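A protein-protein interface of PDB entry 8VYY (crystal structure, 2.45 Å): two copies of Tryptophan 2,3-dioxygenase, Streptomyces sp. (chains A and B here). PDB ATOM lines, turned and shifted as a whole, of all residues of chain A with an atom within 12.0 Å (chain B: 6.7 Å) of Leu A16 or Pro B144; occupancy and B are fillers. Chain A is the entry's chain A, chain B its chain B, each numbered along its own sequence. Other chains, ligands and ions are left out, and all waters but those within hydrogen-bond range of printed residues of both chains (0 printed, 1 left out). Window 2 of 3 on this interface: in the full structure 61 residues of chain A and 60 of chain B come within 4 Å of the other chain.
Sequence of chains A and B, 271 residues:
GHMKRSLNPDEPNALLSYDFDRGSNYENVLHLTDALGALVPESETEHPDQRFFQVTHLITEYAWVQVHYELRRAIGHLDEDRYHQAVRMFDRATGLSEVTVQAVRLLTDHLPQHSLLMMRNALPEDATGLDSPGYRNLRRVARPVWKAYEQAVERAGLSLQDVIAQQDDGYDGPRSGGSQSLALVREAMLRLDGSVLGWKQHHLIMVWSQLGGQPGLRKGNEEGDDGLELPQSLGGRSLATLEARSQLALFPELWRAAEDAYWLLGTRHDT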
ATOM      1  N   LEU A   7     -28.628  -8.376 -11.613  1.00  0.00           N
ATOM      2  CA  LEU A   7     -28.261  -7.270 -12.500  1.00  0.00           C
ATOM      3  C   LEU A   7     -27.562  -6.144 -11.730  1.00  0.00           C
ATOM      4  O   LEU A   7     -27.148  -6.331 -10.579  1.00  0.00           O
ATOM      5  CB  LEU A   7     -29.502  -6.718 -13.230  1.00  0.00           C
ATOM      6  CG  LEU A   7     -30.142  -7.402 -14.450  1.00  0.00           C
ATOM      7  CD1 LEU A   7     -31.249  -8.379 -14.020  1.00  0.00           C
ATOM      8  CD2 LEU A   7     -30.694  -6.369 -15.450  1.00  0.00           C
ATOM      9  N   ASN A   8     -27.435  -4.953 -12.350  1.00  0.00           N
ATOM     10  CA  ASN A   8     -26.696  -3.856 -11.727  1.00  0.00           C
ATOM     11  C   ASN A   8     -26.921  -2.509 -12.419  1.00  0.00           C
ATOM     12  O   ASN A   8     -26.548  -2.349 -13.590  1.00  0.00           O
ATOM     13  CB  ASN A   8     -25.203  -4.196 -11.721  1.00  0.00           C
ATOM     14  CG  ASN A   8     -24.562  -3.994 -10.360  1.00  0.00           C
ATOM     15  OD1 ASN A   8     -24.520  -2.877  -9.845  1.00  0.00           O
ATOM     16  ND2 ASN A   8     -24.056  -5.080  -9.771  1.00  0.00           N
ATOM     17  N   PRO A   9     -27.543  -1.509 -11.744  1.00  0.00           N
ATOM     18  CA  PRO A   9     -27.599  -0.156 -12.327  1.00  0.00           C
ATOM     19  C   PRO A   9     -26.281   0.617 -12.374  1.00  0.00           C
ATOM     20  O   PRO A   9     -26.311   1.790 -12.757  1.00  0.00           O
ATOM     21  CB  PRO A   9     -28.625   0.561 -11.431  1.00  0.00           C
ATOM     22  CG  PRO A   9     -29.565  -0.512 -11.028  1.00  0.00           C
ATOM     23  CD  PRO A   9     -28.658  -1.725 -10.800  1.00  0.00           C
ATOM     24  N   ASP A  10     -25.141   0.020 -12.004  1.00  0.00           N
ATOM     25  CA  ASP A  10     -23.841   0.673 -12.192  1.00  0.00           C
ATOM     26  C   ASP A  10     -22.731  -0.380 -12.262  1.00  0.00           C
ATOM     27  O   ASP A  10     -22.834  -1.440 -11.642  1.00  0.00           O
ATOM     28  CB  ASP A  10     -23.552   1.718 -11.093  1.00  0.00           C
ATOM     29  CG  ASP A  10     -23.698   1.171  -9.668  1.00  0.00           C
ATOM     30  OD1 ASP A  10     -24.529   0.272  -9.424  1.00  0.00           O
ATOM     31  OD2 ASP A  10     -22.982   1.676  -8.777  1.00  0.00           O
ATOM     32  N   GLU A  11     -21.660  -0.086 -13.042  1.00  0.00           N
ATOM     33  CA  GLU A  11     -20.680  -1.137 -13.347  1.00  0.00           C
ATOM     34  C   GLU A  11     -19.323  -0.970 -12.658  1.00  0.00           C
ATOM     35  O   GLU A  11     -18.977  -1.803 -11.809  1.00  0.00           O
ATOM     36  CB  GLU A  11     -20.471  -1.271 -14.863  1.00  0.00           C
ATOM     37  CG  GLU A  11     -21.726  -1.572 -15.650  1.00  0.00           C
ATOM     38  CD  GLU A  11     -22.772  -2.309 -14.834  1.00  0.00           C
ATOM     39  OE1 GLU A  11     -22.473  -3.395 -14.287  1.00  0.00           O
ATOM     40  OE2 GLU A  11     -23.898  -1.781 -14.728  1.00  0.00           O
ATOM     41  N   PRO A  12     -18.496   0.053 -12.988  1.00  0.00           N
ATOM     42  CA  PRO A  12     -17.135   0.064 -12.429  1.00  0.00           C
ATOM     43  C   PRO A  12     -17.060   0.769 -11.080  1.00  0.00           C
ATOM     44  O   PRO A  12     -16.933   1.998 -11.035  1.00  0.00           O
ATOM     45  CB  PRO A  12     -16.325   0.805 -13.505  1.00  0.00           C
ATOM     46  CG  PRO A  12     -17.359   1.643 -14.278  1.00  0.00           C
ATOM     47  CD  PRO A  12     -18.743   1.276 -13.777  1.00  0.00           C
ATOM     48  N   ASN A  13     -17.123   0.021  -9.973  1.00  0.00           N
ATOM     49  CA  ASN A  13     -17.249   0.645  -8.661  1.00  0.00           C
ATOM     50  C   ASN A  13     -16.424  -0.102  -7.615  1.00  0.00           C
ATOM     51  O   ASN A  13     -15.755  -1.105  -7.900  1.00  0.00           O
ATOM     52  CB  ASN A  13     -18.722   0.722  -8.222  1.00  0.00           C
ATOM     53  CG  ASN A  13     -19.418   1.986  -8.709  1.00  0.00           C
ATOM     54  OD1 ASN A  13     -19.935   2.029  -9.827  1.00  0.00           O
ATOM     55  ND2 ASN A  13     -19.426   3.026  -7.873  1.00  0.00           N
ATOM     56  N   ALA A  14     -16.491   0.424  -6.386  1.00  0.00           N
ATOM     57  CA  ALA A  14     -15.872  -0.145  -5.196  1.00  0.00           C
ATOM     58  C   ALA A  14     -16.795  -1.150  -4.515  1.00  0.00           C
ATOM     59  O   ALA A  14     -16.787  -1.259  -3.283  1.00  0.00           O
ATOM     60  CB  ALA A  14     -15.497   0.959  -4.207  1.00  0.00           C
ATOM     61  N   LEU A  15     -17.632  -1.827  -5.310  1.00  0.00           N
ATOM     62  CA  LEU A  15     -18.273  -3.087  -4.937  1.00  0.00           C
ATOM     63  C   LEU A  15     -19.362  -2.924  -3.873  1.00  0.00           C
ATOM     64  O   LEU A  15     -20.492  -3.401  -4.055  1.00  0.00           O
ATOM     65  CB  LEU A  15     -17.205  -4.096  -4.479  1.00  0.00           C
ATOM     66  CG  LEU A  15     -16.332  -4.864  -5.503  1.00  0.00           C
ATOM     67  CD1 LEU A  15     -15.702  -3.979  -6.594  1.00  0.00           C
ATOM     68  CD2 LEU A  15     -15.241  -5.681  -4.790  1.00  0.00           C
ATOM     69  N   LEU A  16     -19.040  -2.267  -2.752  1.00  0.00           N
ATOM     70  CA  LEU A  16     -20.052  -1.882  -1.771  1.00  0.00           C
ATOM     71  C   LEU A  16     -20.896  -0.702  -2.232  1.00  0.00           C
ATOM     72  O   LEU A  16     -21.754  -0.239  -1.467  1.00  0.00           O
ATOM     73  CB  LEU A  16     -19.406  -1.513  -0.435  1.00  0.00           C
ATOM     74  CG  LEU A  16     -18.704  -2.561   0.419  1.00  0.00           C
ATOM     75  CD1 LEU A  16     -17.275  -2.094   0.717  1.00  0.00           C
ATOM     76  CD2 LEU A  16     -19.504  -2.795   1.700  1.00  0.00           C
ATOM     77  N   SER A  17     -20.654  -0.185  -3.436  1.00  0.00           N
ATOM     78  CA  SER A  17     -21.418   0.923  -3.984  1.00  0.00           C
ATOM     79  C   SER A  17     -22.265   0.485  -5.183  1.00  0.00           C
ATOM     80  O   SER A  17     -22.639   1.307  -6.022  1.00  0.00           O
ATOM     81  CB  SER A  17     -20.472   2.073  -4.338  1.00  0.00           C
ATOM     82  OG  SER A  17     -19.876   2.614  -3.158  1.00  0.00           O
ATOM     83  N   TYR A  18     -22.588  -0.810  -5.253  1.00  0.00           N
ATOM     84  CA  TYR A  18     -23.420  -1.425  -6.281  1.00  0.00           C
ATOM     85  C   TYR A  18     -24.905  -1.394  -5.885  1.00  0.00           C
ATOM     86  O   TYR A  18     -25.249  -1.222  -4.715  1.00  0.00           O
ATOM     87  CB  TYR A  18     -23.006  -2.884  -6.496  1.00  0.00           C
ATOM     88  CG  TYR A  18     -21.942  -3.145  -7.542  1.00  0.00           C
ATOM     89  CD1 TYR A  18     -21.823  -2.338  -8.664  1.00  0.00           C
ATOM     90  CD2 TYR A  18     -21.084  -4.246  -7.431  1.00  0.00           C
ATOM     91  CE1 TYR A  18     -20.854  -2.592  -9.633  1.00  0.00           C
ATOM     92  CE2 TYR A  18     -20.114  -4.511  -8.399  1.00  0.00           C
ATOM     93  CZ  TYR A  18     -20.005  -3.680  -9.496  1.00  0.00           C
ATOM     94  OH  TYR A  18     -19.050  -3.931 -10.458  1.00  0.00           O
ATOM     95  N   ASP A  19     -25.779  -1.605  -6.886  1.00  0.00           N
ATOM     96  CA  ASP A  19     -27.232  -1.791  -6.756  1.00  0.00           C
ATOM     97  C   ASP A  19     -27.610  -3.082  -7.501  1.00  0.00           C
ATOM     98  O   ASP A  19     -27.075  -3.326  -8.582  1.00  0.00           O
ATOM     99  CB  ASP A  19     -27.977  -0.526  -7.342  1.00  0.00           C
ATOM    100  CG  ASP A  19     -29.354  -0.233  -6.679  1.00  0.00           C
ATOM    101  OD1 ASP A  19     -30.383  -0.776  -7.171  1.00  0.00           O
ATOM    102  OD2 ASP A  19     -29.427   0.579  -5.712  1.00  0.00           O
ATOM    103  N   PHE A  20     -28.532  -3.918  -6.958  1.00  0.00           N
ATOM    104  CA  PHE A  20     -28.757  -5.281  -7.479  1.00  0.00           C
ATOM    105  C   PHE A  20     -30.238  -5.598  -7.757  1.00  0.00           C
ATOM    106  O   PHE A  20     -31.117  -5.045  -7.097  1.00  0.00           O
ATOM    107  CB  PHE A  20     -28.195  -6.314  -6.483  1.00  0.00           C
ATOM    108  CG  PHE A  20     -26.680  -6.294  -6.346  1.00  0.00           C
ATOM    109  CD1 PHE A  20     -26.065  -5.485  -5.402  1.00  0.00           C
ATOM    110  CD2 PHE A  20     -25.876  -7.109  -7.144  1.00  0.00           C
ATOM    111  CE1 PHE A  20     -24.676  -5.479  -5.258  1.00  0.00           C
ATOM    112  CE2 PHE A  20     -24.484  -7.103  -7.012  1.00  0.00           C
ATOM    113  CZ  PHE A  20     -23.886  -6.285  -6.067  1.00  0.00           C
ATOM    114  N   GLU A  42     -26.797   4.712 -16.285  1.00  0.00           N
ATOM    115  CA  GLU A  42     -25.747   5.653 -15.887  1.00  0.00           C
ATOM    116  C   GLU A  42     -24.756   5.903 -17.015  1.00  0.00           C
ATOM    117  O   GLU A  42     -24.195   7.001 -17.118  1.00  0.00           O
ATOM    118  CB  GLU A  42     -25.022   5.143 -14.645  1.00  0.00           C
ATOM    119  CG  GLU A  42     -25.972   4.739 -13.536  1.00  0.00           C
ATOM    120  CD  GLU A  42     -25.335   4.812 -12.167  1.00  0.00           C
ATOM    121  OE1 GLU A  42     -24.192   5.323 -12.074  1.00  0.00           O
ATOM    122  OE2 GLU A  42     -25.976   4.340 -11.194  1.00  0.00           O
ATOM    123  N   HIS B  68     -29.744   6.068  -2.805  1.00  0.00           N
ATOM    124  CA  HIS B  68     -28.466   5.413  -3.060  1.00  0.00           C
ATOM    125  C   HIS B  68     -27.589   6.249  -3.990  1.00  0.00           C
ATOM    126  O   HIS B  68     -26.440   6.570  -3.662  1.00  0.00           O
ATOM    127  CB  HIS B  68     -28.709   4.030  -3.660  1.00  0.00           C
ATOM    128  CG  HIS B  68     -27.489   3.177  -3.702  1.00  0.00           C
ATOM    129  ND1 HIS B  68     -26.611   3.192  -4.764  1.00  0.00           N
ATOM    130  CD2 HIS B  68     -26.988   2.288  -2.811  1.00  0.00           C
ATOM    131  CE1 HIS B  68     -25.621   2.350  -4.525  1.00  0.00           C
ATOM    132  NE2 HIS B  68     -25.826   1.789  -3.348  1.00  0.00           N
ATOM    133  N   ILE B  75     -20.235  10.578  -1.199  1.00  0.00           N
ATOM    134  CA  ILE B  75     -18.936   9.973  -0.943  1.00  0.00           C
ATOM    135  C   ILE B  75     -17.867  10.649  -1.792  1.00  0.00           C
ATOM    136  O   ILE B  75     -16.790  10.995  -1.294  1.00  0.00           O
ATOM    137  CB  ILE B  75     -18.997   8.457  -1.198  1.00  0.00           C
ATOM    138  CG1 ILE B  75     -19.908   7.783  -0.188  1.00  0.00           C
ATOM    139  CG2 ILE B  75     -17.619   7.844  -1.096  1.00  0.00           C
ATOM    140  CD1 ILE B  75     -20.201   6.307  -0.554  1.00  0.00           C
ATOM    141  N   LEU B  78     -17.137  14.088  -0.346  1.00  0.00           N
ATOM    142  CA  LEU B  78     -16.406  14.008   0.914  1.00  0.00           C
ATOM    143  C   LEU B  78     -14.953  13.605   0.680  1.00  0.00           C
ATOM    144  O   LEU B  78     -14.042  14.154   1.313  1.00  0.00           O
ATOM    145  CB  LEU B  78     -17.092  13.024   1.859  1.00  0.00           C
ATOM    146  CG  LEU B  78     -18.388  13.539   2.492  1.00  0.00           C
ATOM    147  CD1 LEU B  78     -19.075  12.436   3.280  1.00  0.00           C
ATOM    148  CD2 LEU B  78     -18.120  14.752   3.367  1.00  0.00           C
ATOM    149  N   ASP B  79     -14.720  12.649  -0.230  1.00  0.00           N
ATOM    150  CA  ASP B  79     -13.367  12.192  -0.520  1.00  0.00           C
ATOM    151  C   ASP B  79     -12.507  13.286  -1.158  1.00  0.00           C
ATOM    152  O   ASP B  79     -11.276  13.196  -1.089  1.00  0.00           O
ATOM    153  CB  ASP B  79     -13.416  10.948  -1.419  1.00  0.00           C
ATOM    154  CG  ASP B  79     -13.801   9.682  -0.648  1.00  0.00           C
ATOM    155  OD1 ASP B  79     -13.752   9.708   0.603  1.00  0.00           O
ATOM    156  OD2 ASP B  79     -14.138   8.652  -1.279  1.00  0.00           O
ATOM    157  N   ASN B 137     -29.469  -2.227  -0.528  1.00  0.00           N
ATOM    158  CA  ASN B 137     -28.397  -1.402  -1.064  1.00  0.00           C
ATOM    159  C   ASN B 137     -28.162  -0.163  -0.218  1.00  0.00           C
ATOM    160  O   ASN B 137     -27.027   0.310  -0.117  1.00  0.00           O
ATOM    161  CB  ASN B 137     -28.705  -1.027  -2.509  1.00  0.00           C
ATOM    162  CG  ASN B 137     -28.630  -2.217  -3.432  1.00  0.00           C
ATOM    163  OD1 ASN B 137     -27.622  -2.925  -3.453  1.00  0.00           O
ATOM    164  ND2 ASN B 137     -29.697  -2.466  -4.185  1.00  0.00           N
ATOM    165  N   ARG B 139     -28.488  -0.142   2.970  1.00  0.00           N
ATOM    166  CA  ARG B 139     -27.753  -0.664   4.115  1.00  0.00           C
ATOM    167  C   ARG B 139     -26.273  -0.863   3.781  1.00  0.00           C
ATOM    168  O   ARG B 139     -25.400  -0.515   4.587  1.00  0.00           O
ATOM    169  CB  ARG B 139     -28.409  -1.965   4.567  1.00  0.00           C
ATOM    170  CG  ARG B 139     -28.308  -2.239   6.034  1.00  0.00           C
ATOM    171  CD  ARG B 139     -29.552  -1.824   6.814  1.00  0.00           C
ATOM    172  NE  ARG B 139     -29.171  -1.662   8.212  1.00  0.00           N
ATOM    173  CZ  ARG B 139     -29.204  -0.517   8.877  1.00  0.00           C
ATOM    174  NH1 ARG B 139     -29.732   0.576   8.351  1.00  0.00           N
ATOM    175  NH2 ARG B 139     -28.698  -0.471  10.101  1.00  0.00           N
ATOM    176  N   ARG B 140     -25.973  -1.402   2.591  1.00  0.00           N
ATOM    177  CA  ARG B 140     -24.588  -1.584   2.152  1.00  0.00           C
ATOM    178  C   ARG B 140     -23.844  -0.260   2.066  1.00  0.00           C
ATOM    179  O   ARG B 140     -22.735  -0.123   2.588  1.00  0.00           O
ATOM    180  CB  ARG B 140     -24.543  -2.253   0.782  1.00  0.00           C
ATOM    181  CG  ARG B 140     -24.314  -3.736   0.780  1.00  0.00           C
ATOM    182  CD  ARG B 140     -23.751  -4.185  -0.580  1.00  0.00           C
ATOM    183  NE  ARG B 140     -24.802  -4.496  -1.541  1.00  0.00           N
ATOM    184  CZ  ARG B 140     -25.729  -5.429  -1.358  1.00  0.00           C
ATOM    185  NH1 ARG B 140     -25.735  -6.201  -0.281  1.00  0.00           N
ATOM    186  NH2 ARG B 140     -26.679  -5.594  -2.279  1.00  0.00           N
ATOM    187  N   VAL B 141     -24.423   0.716   1.369  1.00  0.00           N
ATOM    188  CA  VAL B 141     -23.724   1.960   1.090  1.00  0.00           C
ATOM    189  C   VAL B 141     -23.525   2.814   2.328  1.00  0.00           C
ATOM    190  O   VAL B 141     -22.718   3.747   2.293  1.00  0.00           O
ATOM    191  CB  VAL B 141     -24.494   2.754   0.017  1.00  0.00           C
ATOM    192  CG1 VAL B 141     -25.679   3.470   0.651  1.00  0.00           C
ATOM    193  CG2 VAL B 141     -23.555   3.731  -0.707  1.00  0.00           C
ATOM    194  N   ALA B 142     -24.226   2.511   3.423  1.00  0.00           N
ATOM    195  CA  ALA B 142     -24.122   3.340   4.621  1.00  0.00           C
ATOM    196  C   ALA B 142     -22.727   3.271   5.227  1.00  0.00           C
ATOM    197  O   ALA B 142     -22.243   4.261   5.787  1.00  0.00           O
ATOM    198  CB  ALA B 142     -25.161   2.912   5.667  1.00  0.00           C
ATOM    199  N   ARG B 143     -22.088   2.094   5.180  1.00  0.00           N
ATOM    200  CA  ARG B 143     -20.740   1.980   5.736  1.00  0.00           C
ATOM    201  C   ARG B 143     -19.740   2.809   4.938  1.00  0.00           C
ATOM    202  O   ARG B 143     -19.035   3.635   5.545  1.00  0.00           O
ATOM    203  CB  ARG B 143     -20.321   0.506   5.829  1.00  0.00           C
ATOM    204  CG  ARG B 143     -21.038  -0.312   6.910  1.00  0.00           C
ATOM    205  CD  ARG B 143     -20.709   0.163   8.329  1.00  0.00           C
ATOM    206  NE  ARG B 143     -21.618   1.221   8.764  1.00  0.00           N
ATOM    207  CZ  ARG B 143     -21.303   2.173   9.632  1.00  0.00           C
ATOM    208  NH1 ARG B 143     -20.113   2.222  10.205  1.00  0.00           N
ATOM    209  NH2 ARG B 143     -22.209   3.097   9.936  1.00  0.00           N
ATOM    210  N   PRO B 144     -19.639   2.675   3.601  1.00  0.00           N
ATOM    211  CA  PRO B 144     -18.753   3.589   2.862  1.00  0.00           C
ATOM    212  C   PRO B 144     -19.075   5.048   3.107  1.00  0.00           C
ATOM    213  O   PRO B 144     -18.156   5.877   3.158  1.00  0.00           O
ATOM    214  CB  PRO B 144     -19.007   3.219   1.393  1.00  0.00           C
ATOM    215  CG  PRO B 144     -19.592   1.919   1.405  1.00  0.00           C
ATOM    216  CD  PRO B 144     -20.293   1.721   2.689  1.00  0.00           C
ATOM    217  N   VAL B 145     -20.366   5.391   3.222  1.00  0.00           N
ATOM    218  CA  VAL B 145     -20.739   6.788   3.435  1.00  0.00           C
ATOM    219  C   VAL B 145     -20.154   7.286   4.745  1.00  0.00           C
ATOM    220  O   VAL B 145     -19.539   8.362   4.806  1.00  0.00           O
ATOM    221  CB  VAL B 145     -22.269   6.965   3.412  1.00  0.00           C
ATOM    222  CG1 VAL B 145     -22.644   8.351   3.926  1.00  0.00           C
ATOM    223  CG2 VAL B 145     -22.794   6.798   2.015  1.00  0.00           C
ATOM    224  N   TRP B 146     -20.342   6.510   5.815  1.00  0.00           N
ATOM    225  CA  TRP B 146     -19.817   6.910   7.110  1.00  0.00           C
ATOM    226  C   TRP B 146     -18.286   6.984   7.094  1.00  0.00           C
ATOM    227  O   TRP B 146     -17.696   7.927   7.638  1.00  0.00           O
ATOM    228  CB  TRP B 146     -20.284   5.948   8.204  1.00  0.00           C
ATOM    229  CG  TRP B 146     -19.575   6.325   9.447  1.00  0.00           C
ATOM    230  CD1 TRP B 146     -18.515   5.686  10.024  1.00  0.00           C
ATOM    231  CD2 TRP B 146     -19.797   7.512  10.212  1.00  0.00           C
ATOM    232  NE1 TRP B 146     -18.096   6.388  11.120  1.00  0.00           N
ATOM    233  CE2 TRP B 146     -18.865   7.514  11.253  1.00  0.00           C
ATOM    234  CE3 TRP B 146     -20.725   8.553  10.131  1.00  0.00           C
ATOM    235  CZ2 TRP B 146     -18.821   8.523  12.205  1.00  0.00           C
ATOM    236  CZ3 TRP B 146     -20.688   9.545  11.080  1.00  0.00           C
ATOM    237  CH2 TRP B 146     -19.741   9.524  12.105  1.00  0.00           C
ATOM    238  N   LYS B 147     -17.628   5.990   6.486  1.00  0.00           N
ATOM    239  CA  LYS B 147     -16.174   6.007   6.363  1.00  0.00           C
ATOM    240  C   LYS B 147     -15.687   7.296   5.710  1.00  0.00           C
ATOM    241  O   LYS B 147     -14.743   7.935   6.195  1.00  0.00           O
ATOM    242  CB  LYS B 147     -15.701   4.790   5.564  1.00  0.00           C
ATOM    243  CG  LYS B 147     -14.627   3.967   6.236  1.00  0.00           C
ATOM    244  CD  LYS B 147     -15.124   3.367   7.553  1.00  0.00           C
ATOM    245  CE  LYS B 147     -13.968   3.153   8.537  1.00  0.00           C
ATOM    246  NZ  LYS B 147     -14.457   2.967   9.928  1.00  0.00           N
ATOM    247  N   ALA B 148     -16.330   7.697   4.606  1.00  0.00           N
ATOM    248  CA  ALA B 148     -15.915   8.913   3.913  1.00  0.00           C
ATOM    249  C   ALA B 148     -16.078  10.143   4.799  1.00  0.00           C
ATOM    250  O   ALA B 148     -15.225  11.034   4.793  1.00  0.00           O
ATOM    251  CB  ALA B 148     -16.704   9.081   2.612  1.00  0.00           C
ATOM    252  N   TYR B 149     -17.166  10.217   5.569  1.00  0.00           N
ATOM    253  CA  TYR B 149     -17.323  11.363   6.460  1.00  0.00           C
ATOM    254  C   TYR B 149     -16.278  11.341   7.569  1.00  0.00           C
ATOM    255  O   TYR B 149     -15.674  12.376   7.882  1.00  0.00           O
ATOM    256  CB  TYR B 149     -18.729  11.397   7.065  1.00  0.00           C
ATOM    257  CG  TYR B 149     -18.887  12.553   8.004  1.00  0.00           C
ATOM    258  CD1 TYR B 149     -18.851  13.851   7.525  1.00  0.00           C
ATOM    259  CD2 TYR B 149     -19.027  12.362   9.371  1.00  0.00           C
ATOM    260  CE1 TYR B 149     -18.983  14.937   8.370  1.00  0.00           C
ATOM    261  CE2 TYR B 149     -19.145  13.449  10.235  1.00  0.00           C
ATOM    262  CZ  TYR B 149     -19.119  14.735   9.719  1.00  0.00           C
ATOM    263  OH  TYR B 149     -19.232  15.839  10.531  1.00  0.00           O
ATOM    264  N   GLN B 151     -13.262   9.925   7.669  1.00  0.00           N
ATOM    265  CA  GLN B 151     -11.938  10.297   7.171  1.00  0.00           C
ATOM    266  C   GLN B 151     -11.834  11.796   6.916  1.00  0.00           C
ATOM    267  O   GLN B 151     -10.785  12.399   7.168  1.00  0.00           O
ATOM    268  CB  GLN B 151     -11.596   9.507   5.906  1.00  0.00           C
ATOM    269  CG  GLN B 151     -11.409   8.020   6.187  1.00  0.00           C
ATOM    270  CD  GLN B 151     -11.507   7.156   4.928  1.00  0.00           C
ATOM    271  OE1 GLN B 151     -10.958   6.052   4.882  1.00  0.00           O
ATOM    272  NE2 GLN B 151     -12.193   7.663   3.894  1.00  0.00           N
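The backbone carbonyl oxygen (O) of Tyr A18 is in hydrogen-bond range of a ring nitrogen (NE2) of His B68, at 3.4 Å. The backbone carbonyl oxygen (O) of Tyr A18 sits close to the side-chain amide oxygen (OD1) of Asn B137. The side-chain carboxylate (OD2) of Asp A19 sits close to the side-chain amide nitrogen (ND2) of Asn B137. N of Phe A20 sits close to ND2 of Asn B137, at 3.3 Å.
OD1 of Asn A8 lies close to O of Asp A19 (2.9 Å). N of Asp A19 sits at hydrogen-bond distance from OD1 of Asp A10 (3.4 Å). O of Glu A11 lies within hydrogen-bond range of OH of Tyr A18 (2.5 Å). OD1 of Asn B137 sits at hydrogen-bond distance from NH2 of Arg B140 (3.1 Å).
Val B141 touches Leu A16. CB of Leu A16 touches CG of Pro B144, 3.9 Å away. His B68 touches Ser A17. His B68 touches Asp A19. Phe A20 touches Arg B140 (CD1 to NH2, 3.2 Å).
Pro B144 touches just one residue of chain A: Leu A16. No residue of chain A comes within 4 Å of Ile B75. Of chain A, only Phe A20 (3.2 Å) comes within 4 Å of Arg B140. Of chain A, only Leu A16 (3.9 Å) comes within 4 Å of Val B141. No residue of chain A comes within 4 Å of Ala B148. Of the printed residues of chain B, Asp A19 touches His B68 and Asn B137. Of the printed residues of chain B, Phe A20 touches Asn B137 (3.3 Å) and Arg B140 (3.2 Å). Of the printed residues of chain B, Tyr A18 touches His B68 (3.4 Å) and Asn B137 (3.2 Å). Of the printed residues of chain B, Ser A17 touches His B68 (3.5 Å). Of the printed residues of chain A, Asn B137 touches Tyr A18, Asp A19 and Phe A20. Asp A10 touches none of the printed residues of chain B. Glu A42 touches none of the printed residues of chain B. The nearest residue of chain A that does not touch Pro B144 is Ser A17 (4.6 Å).
Hydrophobic or aromatic side chains of chain B within 4 Å of the printed part of chain A: His B68 and Pro B144. Among the printed residues, no Asp or Glu carboxylate lies within 4 Å of a Lys or Arg side-chain nitrogen of the other chain.
No position is printed for both chains. Of the 9 pairs that touch across the chains among the printed residues, none has its exchanged pair printed and touching as well.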
